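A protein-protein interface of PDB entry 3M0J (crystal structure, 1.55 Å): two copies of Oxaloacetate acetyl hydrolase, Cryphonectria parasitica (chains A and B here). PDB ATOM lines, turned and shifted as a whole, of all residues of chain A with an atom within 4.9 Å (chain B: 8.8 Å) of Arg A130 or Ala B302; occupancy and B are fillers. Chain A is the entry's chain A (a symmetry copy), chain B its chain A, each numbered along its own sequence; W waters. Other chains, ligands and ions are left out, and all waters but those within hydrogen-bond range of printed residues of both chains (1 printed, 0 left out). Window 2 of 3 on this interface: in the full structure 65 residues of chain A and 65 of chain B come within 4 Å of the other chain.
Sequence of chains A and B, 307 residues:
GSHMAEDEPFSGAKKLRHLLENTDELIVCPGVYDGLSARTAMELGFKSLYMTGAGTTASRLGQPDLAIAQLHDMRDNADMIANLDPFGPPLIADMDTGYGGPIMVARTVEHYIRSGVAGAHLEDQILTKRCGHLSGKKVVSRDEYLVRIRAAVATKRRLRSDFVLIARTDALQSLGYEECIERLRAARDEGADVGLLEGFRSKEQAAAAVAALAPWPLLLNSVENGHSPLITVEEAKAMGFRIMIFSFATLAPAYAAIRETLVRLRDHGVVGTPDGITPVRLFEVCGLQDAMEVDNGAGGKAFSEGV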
ATOM      1  N   ASP A  65      25.153  24.203  20.243  1.00  0.00           N
ATOM      2  CA  ASP A  65      23.814  24.789  20.272  1.00  0.00           C
ATOM      3  C   ASP A  65      23.636  25.550  21.581  1.00  0.00           C
ATOM      4  O   ASP A  65      22.914  25.103  22.487  1.00  0.00           O
ATOM      5  CB  ASP A  65      22.799  23.653  20.147  1.00  0.00           C
ATOM      6  CG  ASP A  65      21.366  24.141  20.007  1.00  0.00           C
ATOM      7  OD1 ASP A  65      21.135  25.272  19.528  1.00  0.00           O
ATOM      8  OD2 ASP A  65      20.473  23.363  20.370  1.00  0.00           O
ATOM      9  N   LEU A  66      24.332  26.685  21.693  1.00  0.00           N
ATOM     10  CA  LEU A  66      24.330  27.466  22.928  1.00  0.00           C
ATOM     11  C   LEU A  66      23.974  28.929  22.653  1.00  0.00           C
ATOM     12  O   LEU A  66      24.656  29.841  23.131  1.00  0.00           O
ATOM     13  CB  LEU A  66      25.710  27.394  23.597  1.00  0.00           C
ATOM     14  CG  LEU A  66      26.146  26.022  24.131  1.00  0.00           C
ATOM     15  CD1 LEU A  66      27.553  26.100  24.717  1.00  0.00           C
ATOM     16  CD2 LEU A  66      25.170  25.506  25.171  1.00  0.00           C
ATOM     17  N   GLN A 125      12.679  28.959  26.679  1.00  0.00           N
ATOM     18  CA  GLN A 125      13.991  29.030  27.320  1.00  0.00           C
ATOM     19  C   GLN A 125      14.422  30.475  27.576  1.00  0.00           C
ATOM     20  O   GLN A 125      13.977  31.399  26.882  1.00  0.00           O
ATOM     21  CB  GLN A 125      15.040  28.299  26.481  1.00  0.00           C
ATOM     22  CG  GLN A 125      14.837  26.790  26.430  1.00  0.00           C
ATOM     23  CD  GLN A 125      16.075  26.050  25.968  1.00  0.00           C
ATOM     24  OE1 GLN A 125      16.013  25.193  25.078  1.00  0.00           O
ATOM     25  NE2 GLN A 125      17.210  26.382  26.554  1.00  0.00           N
ATOM     26  N   THR A 128      19.719  33.101  26.849  1.00  0.00           N
ATOM     27  CA  THR A 128      20.959  32.339  26.804  1.00  0.00           C
ATOM     28  C   THR A 128      20.616  30.848  26.898  1.00  0.00           C
ATOM     29  O   THR A 128      20.899  30.188  27.895  1.00  0.00           O
ATOM     30  CB  THR A 128      21.916  32.770  27.921  1.00  0.00           C
ATOM     31  OG1 THR A 128      21.249  32.689  29.187  1.00  0.00           O
ATOM     32  CG2 THR A 128      22.352  34.208  27.701  1.00  0.00           C
ATOM     33  N   LYS A 129      19.997  30.340  25.835  1.00  0.00           N
ATOM     34  CA  LYS A 129      19.434  28.984  25.778  1.00  0.00           C
ATOM     35  C   LYS A 129      20.464  27.885  25.496  1.00  0.00           C
ATOM     36  O   LYS A 129      21.656  28.146  25.323  1.00  0.00           O
ATOM     37  CB  LYS A 129      18.353  28.927  24.699  1.00  0.00           C
ATOM     38  CG  LYS A 129      18.910  29.163  23.298  1.00  0.00           C
ATOM     39  CD  LYS A 129      18.061  28.511  22.230  1.00  0.00           C
ATOM     40  CE  LYS A 129      18.246  26.987  22.221  1.00  0.00           C
ATOM     41  NZ  LYS A 129      17.153  26.355  21.418  1.00  0.00           N
ATOM     42  N   ARG A 130      19.981  26.649  25.422  1.00  0.00           N
ATOM     43  CA  ARG A 130      20.840  25.498  25.163  1.00  0.00           C
ATOM     44  C   ARG A 130      20.011  24.360  24.593  1.00  0.00           C
ATOM     45  O   ARG A 130      18.790  24.326  24.772  1.00  0.00           O
ATOM     46  CB  ARG A 130      21.558  25.040  26.442  1.00  0.00           C
ATOM     47  CG  ARG A 130      20.659  24.390  27.493  1.00  0.00           C
ATOM     48  CD  ARG A 130      21.419  24.177  28.809  1.00  0.00           C
ATOM     49  NE  ARG A 130      21.909  25.440  29.366  1.00  0.00           N
ATOM     50  CZ  ARG A 130      22.745  25.540  30.397  1.00  0.00           C
ATOM     51  NH1 ARG A 130      23.198  24.448  31.005  1.00  0.00           N
ATOM     52  NH2 ARG A 130      23.133  26.738  30.824  1.00  0.00           N
ATOM     53  N   CYS A 131      20.670  23.431  23.903  1.00  0.00           N
ATOM     54  CA  CYS A 131      19.980  22.255  23.368  1.00  0.00           C
ATOM     55  C   CYS A 131      19.075  21.654  24.448  1.00  0.00           C
ATOM     56  O   CYS A 131      19.497  21.488  25.592  1.00  0.00           O
ATOM     57  CB  CYS A 131      21.006  21.217  22.908  1.00  0.00           C
ATOM     58  SG  CYS A 131      20.277  19.649  22.376  1.00  0.00           S
ATOM     59  N   GLY A 132      17.835  21.332  24.082  1.00  0.00           N
ATOM     60  CA  GLY A 132      16.831  20.907  25.044  1.00  0.00           C
ATOM     61  C   GLY A 132      17.142  19.616  25.782  1.00  0.00           C
ATOM     62  O   GLY A 132      16.483  19.278  26.760  1.00  0.00           O
ATOM     63  N   LEU A 134      20.201  19.053  27.016  1.00  0.00           N
ATOM     64  CA  LEU A 134      21.264  19.342  27.974  1.00  0.00           C
ATOM     65  C   LEU A 134      20.677  19.751  29.326  1.00  0.00           C
ATOM     66  O   LEU A 134      19.627  20.393  29.392  1.00  0.00           O
ATOM     67  CB  LEU A 134      22.179  20.450  27.460  1.00  0.00           C
ATOM     68  CG  LEU A 134      22.951  20.267  26.155  1.00  0.00           C
ATOM     69  CD1 LEU A 134      23.752  21.528  25.865  1.00  0.00           C
ATOM     70  CD2 LEU A 134      23.856  19.063  26.212  1.00  0.00           C
ATOM     71  N   SER A 135      21.356  19.373  30.404  1.00  0.00           N
ATOM     72  CA  SER A 135      20.903  19.727  31.746  1.00  0.00           C
ATOM     73  C   SER A 135      21.228  21.181  32.064  1.00  0.00           C
ATOM     74  O   SER A 135      21.980  21.827  31.335  1.00  0.00           O
ATOM     75  CB  SER A 135      21.542  18.809  32.789  1.00  0.00           C
ATOM     76  OG  SER A 135      21.260  17.454  32.490  1.00  0.00           O
ATOM     77  N   GLY A 136      20.677  21.683  33.167  1.00  0.00           N
ATOM     78  CA  GLY A 136      20.865  23.070  33.558  1.00  0.00           C
ATOM     79  C   GLY A 136      20.052  24.037  32.716  1.00  0.00           C
ATOM     80  O   GLY A 136      20.406  25.213  32.599  1.00  0.00           O
ATOM     81  N   LYS A 137      18.953  23.544  32.144  1.00  0.00           N
ATOM     82  CA  LYS A 137      18.132  24.302  31.194  1.00  0.00           C
ATOM     83  C   LYS A 137      16.978  25.041  31.868  1.00  0.00           C
ATOM     84  O   LYS A 137      16.010  24.418  32.308  1.00  0.00           O
ATOM     85  CB  LYS A 137      17.580  23.345  30.122  1.00  0.00           C
ATOM     86  CG  LYS A 137      16.713  23.995  29.061  1.00  0.00           C
ATOM     87  CD  LYS A 137      16.270  22.965  28.018  1.00  0.00           C
ATOM     88  CE  LYS A 137      15.443  21.855  28.664  1.00  0.00           C
ATOM     89  NZ  LYS A 137      14.676  21.049  27.652  1.00  0.00           N
ATOM     90  N   PHE B 283      28.347  18.275  20.007  1.00  0.00           N
ATOM     91  CA  PHE B 283      28.692  19.575  20.566  1.00  0.00           C
ATOM     92  C   PHE B 283      30.166  19.595  21.000  1.00  0.00           C
ATOM     93  O   PHE B 283      30.873  20.580  20.805  1.00  0.00           O
ATOM     94  CB  PHE B 283      27.763  19.936  21.730  1.00  0.00           C
ATOM     95  CG  PHE B 283      26.306  19.995  21.350  1.00  0.00           C
ATOM     96  CD1 PHE B 283      25.918  20.452  20.099  1.00  0.00           C
ATOM     97  CD2 PHE B 283      25.324  19.612  22.252  1.00  0.00           C
ATOM     98  CE1 PHE B 283      24.568  20.499  19.742  1.00  0.00           C
ATOM     99  CE2 PHE B 283      23.979  19.675  21.915  1.00  0.00           C
ATOM    100  CZ  PHE B 283      23.599  20.117  20.653  1.00  0.00           C
ATOM    101  N   LEU B 288      32.179  22.528  22.410  1.00  0.00           N
ATOM    102  CA  LEU B 288      31.435  22.663  23.667  1.00  0.00           C
ATOM    103  C   LEU B 288      32.335  23.042  24.849  1.00  0.00           C
ATOM    104  O   LEU B 288      32.030  23.956  25.609  1.00  0.00           O
ATOM    105  CB  LEU B 288      30.679  21.366  23.984  1.00  0.00           C
ATOM    106  CG  LEU B 288      29.865  21.410  25.275  1.00  0.00           C
ATOM    107  CD1 LEU B 288      28.819  22.515  25.176  1.00  0.00           C
ATOM    108  CD2 LEU B 288      29.212  20.056  25.585  1.00  0.00           C
ATOM    109  N   ALA B 291      33.415  26.606  24.953  1.00  0.00           N
ATOM    110  CA  ALA B 291      32.314  27.500  25.292  1.00  0.00           C
ATOM    111  C   ALA B 291      32.012  27.481  26.783  1.00  0.00           C
ATOM    112  O   ALA B 291      31.807  28.519  27.397  1.00  0.00           O
ATOM    113  CB  ALA B 291      31.067  27.131  24.500  1.00  0.00           C
ATOM    114  N   MET B 292      31.993  26.293  27.372  1.00  0.00           N
ATOM    115  CA  MET B 292      31.703  26.183  28.792  1.00  0.00           C
ATOM    116  C   MET B 292      32.808  26.838  29.618  1.00  0.00           C
ATOM    117  O   MET B 292      32.546  27.427  30.663  1.00  0.00           O
ATOM    118  CB  MET B 292      31.533  24.722  29.193  1.00  0.00           C
ATOM    119  CG  MET B 292      30.221  24.104  28.753  1.00  0.00           C
ATOM    120  SD  MET B 292      30.173  22.350  29.186  1.00  0.00           S
ATOM    121  CE  MET B 292      28.416  22.107  29.438  1.00  0.00           C
ATOM    122  N   VAL B 294      34.653  29.410  28.657  1.00  0.00           N
ATOM    123  CA  VAL B 294      34.406  30.842  28.571  1.00  0.00           C
ATOM    124  C   VAL B 294      33.395  31.273  29.625  1.00  0.00           C
ATOM    125  O   VAL B 294      33.623  32.245  30.355  1.00  0.00           O
ATOM    126  CB  VAL B 294      33.903  31.259  27.174  1.00  0.00           C
ATOM    127  CG1 VAL B 294      33.384  32.694  27.215  1.00  0.00           C
ATOM    128  CG2 VAL B 294      35.016  31.111  26.155  1.00  0.00           C
ATOM    129  N   ASP B 295      32.284  30.551  29.728  1.00  0.00           N
ATOM    130  CA  ASP B 295      31.270  30.945  30.700  1.00  0.00           C
ATOM    131  C   ASP B 295      31.808  30.821  32.117  1.00  0.00           C
ATOM    132  O   ASP B 295      31.647  31.723  32.948  1.00  0.00           O
ATOM    133  CB  ASP B 295      29.990  30.116  30.554  1.00  0.00           C
ATOM    134  CG  ASP B 295      28.897  30.575  31.507  1.00  0.00           C
ATOM    135  OD1 ASP B 295      28.073  31.424  31.102  1.00  0.00           O
ATOM    136  OD2 ASP B 295      28.881  30.120  32.678  1.00  0.00           O
ATOM    137  N   ASN B 296      32.429  29.686  32.401  1.00  0.00           N
ATOM    138  CA  ASN B 296      32.924  29.438  33.742  1.00  0.00           C
ATOM    139  C   ASN B 296      34.016  30.431  34.114  1.00  0.00           C
ATOM    140  O   ASN B 296      34.023  30.978  35.218  1.00  0.00           O
ATOM    141  CB  ASN B 296      33.443  28.003  33.867  1.00  0.00           C
ATOM    142  CG  ASN B 296      34.082  27.735  35.219  1.00  0.00           C
ATOM    143  OD1 ASN B 296      33.407  27.719  36.248  1.00  0.00           O
ATOM    144  ND2 ASN B 296      35.393  27.530  35.221  1.00  0.00           N
ATOM    145  N   GLY B 297      34.935  30.671  33.186  1.00  0.00           N
ATOM    146  CA  GLY B 297      36.050  31.559  33.450  1.00  0.00           C
ATOM    147  C   GLY B 297      35.622  32.996  33.686  1.00  0.00           C
ATOM    148  O   GLY B 297      36.320  33.755  34.357  1.00  0.00           O
ATOM    149  N   GLY B 299      33.100  33.929  35.332  1.00  0.00           N
ATOM    150  CA  GLY B 299      32.397  34.045  36.595  1.00  0.00           C
ATOM    151  C   GLY B 299      30.942  33.677  36.438  1.00  0.00           C
ATOM    152  O   GLY B 299      30.151  33.824  37.368  1.00  0.00           O
ATOM    153  N   GLY B 300      30.586  33.212  35.246  1.00  0.00           N
ATOM    154  CA  GLY B 300      29.259  32.682  35.001  1.00  0.00           C
ATOM    155  C   GLY B 300      29.089  31.331  35.673  1.00  0.00           C
ATOM    156  O   GLY B 300      30.067  30.634  35.969  1.00  0.00           O
ATOM    157  N   LYS B 301      27.840  30.963  35.923  1.00  0.00           N
ATOM    158  CA  LYS B 301      27.529  29.676  36.529  1.00  0.00           C
ATOM    159  C   LYS B 301      26.514  28.906  35.685  1.00  0.00           C
ATOM    160  O   LYS B 301      25.778  28.061  36.198  1.00  0.00           O
ATOM    161  CB  LYS B 301      27.006  29.876  37.954  1.00  0.00           C
ATOM    162  CG  LYS B 301      25.953  30.967  38.075  1.00  0.00           C
ATOM    163  CD  LYS B 301      25.677  31.312  39.532  1.00  0.00           C
ATOM    164  CE  LYS B 301      24.543  32.315  39.666  1.00  0.00           C
ATOM    165  NZ  LYS B 301      24.898  33.627  39.063  1.00  0.00           N
ATOM    166  N   ALA B 302      26.490  29.195  34.387  1.00  0.00           N
ATOM    167  CA  ALA B 302      25.533  28.566  33.484  1.00  0.00           C
ATOM    168  C   ALA B 302      25.860  27.094  33.276  1.00  0.00           C
ATOM    169  O   ALA B 302      24.965  26.277  33.043  1.00  0.00           O
ATOM    170  CB  ALA B 302      25.507  29.298  32.140  1.00  0.00           C
ATOM    171  N   PHE B 303      27.149  26.766  33.357  1.00  0.00           N
ATOM    172  CA  PHE B 303      27.634  25.411  33.089  1.00  0.00           C
ATOM    173  C   PHE B 303      28.528  24.900  34.211  1.00  0.00           C
ATOM    174  O   PHE B 303      28.381  23.767  34.663  1.00  0.00           O
ATOM    175  CB  PHE B 303      28.435  25.369  31.787  1.00  0.00           C
ATOM    176  CG  PHE B 303      27.688  25.868  30.595  1.00  0.00           C
ATOM    177  CD1 PHE B 303      27.900  27.148  30.117  1.00  0.00           C
ATOM    178  CD2 PHE B 303      26.788  25.052  29.934  1.00  0.00           C
ATOM    179  CE1 PHE B 303      27.218  27.608  29.013  1.00  0.00           C
ATOM    180  CE2 PHE B 303      26.108  25.510  28.825  1.00  0.00           C
ATOM    181  CZ  PHE B 303      26.323  26.787  28.368  1.00  0.00           C
HETATM  182  O   HOH W   1      24.810  22.793  33.329  1.00  0.00           O
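NH2 of Arg A130 lies within hydrogen-bond range of O of Ala B302 (2.9 Å).
The backbone NH (N) of Leu B288 sits at hydrogen-bond distance from the backbone carbonyl oxygen (O) of Phe B283 (2.8 Å). OD2 of Asp B295 sits at hydrogen-bond distance from N of Ala B302. The backbone carbonyl oxygen (O) of Asp A65 is in hydrogen-bond range of the backbone NH (N) of Cys A131 (3.1 Å). O of Arg A130 sits close to OE1 of Gln A125. NH1 of Arg A130 lies within hydrogen-bond range of O of Ser A135, 2.9 Å away. NH1 of Arg A130 lies close to O of Gly A136 (3.3 Å).
CB of Asp A65 touches CE1 of Phe B283 (3.6 Å). CD1 of Leu B288 touches CD1 of Leu A66, at 3.8 Å. CD1 of Leu A66 touches CB of Ala B291, at 3.7 Å. Leu A66 touches Phe B303 (CD2 to CZ, 3.6 Å). Arg A130 touches Phe B303. Phe B283 touches Cys A131 (CE2 to CB, 3.5 Å).
Of chain B, only Ala B302 (2.9 Å) and Phe B303 (3.7 Å) come within 4 Å of Arg A130. Printed residues of chain A within 4 Å of Ala B302: Arg A130 (2.9 Å). Gly A136 touches none of the printed residues of chain B. Of the printed residues of chain A, Ala B291 touches Leu A66 (3.7 Å). Of the printed residues of chain B, Cys A131 touches Phe B283 (3.5 Å). Of the printed residues of chain A, Phe B283 touches Asp A65 (3.6 Å) and Cys A131 (3.5 Å). Of the printed residues of chain A, Leu B288 touches Leu A66 (3.8 Å). The nearest printed residue of chain B that does not touch Cys A131 is Phe B303 (7.6 Å).
Hydrophobic or aromatic side chains of chain A within 4 Å of the printed part of chain B: Leu A66. Of the 13 printed residues of chain B, 5 touch a printed residue of chain A. Among the printed residues, 7 pairs touch across the chains. Among the printed residues, no Asp or Glu carboxylate lies within 4 Å of a Lys or Arg side-chain nitrogen of the other chain.
No position is printed for both chains. Of the 7 pairs that touch across the chains among the printed residues, none has its exchanged pair printed and touching as well.
Water W1 bridges the guanidinium group of Arg A130 and the backbone carbonyl oxygen of Ala B302.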
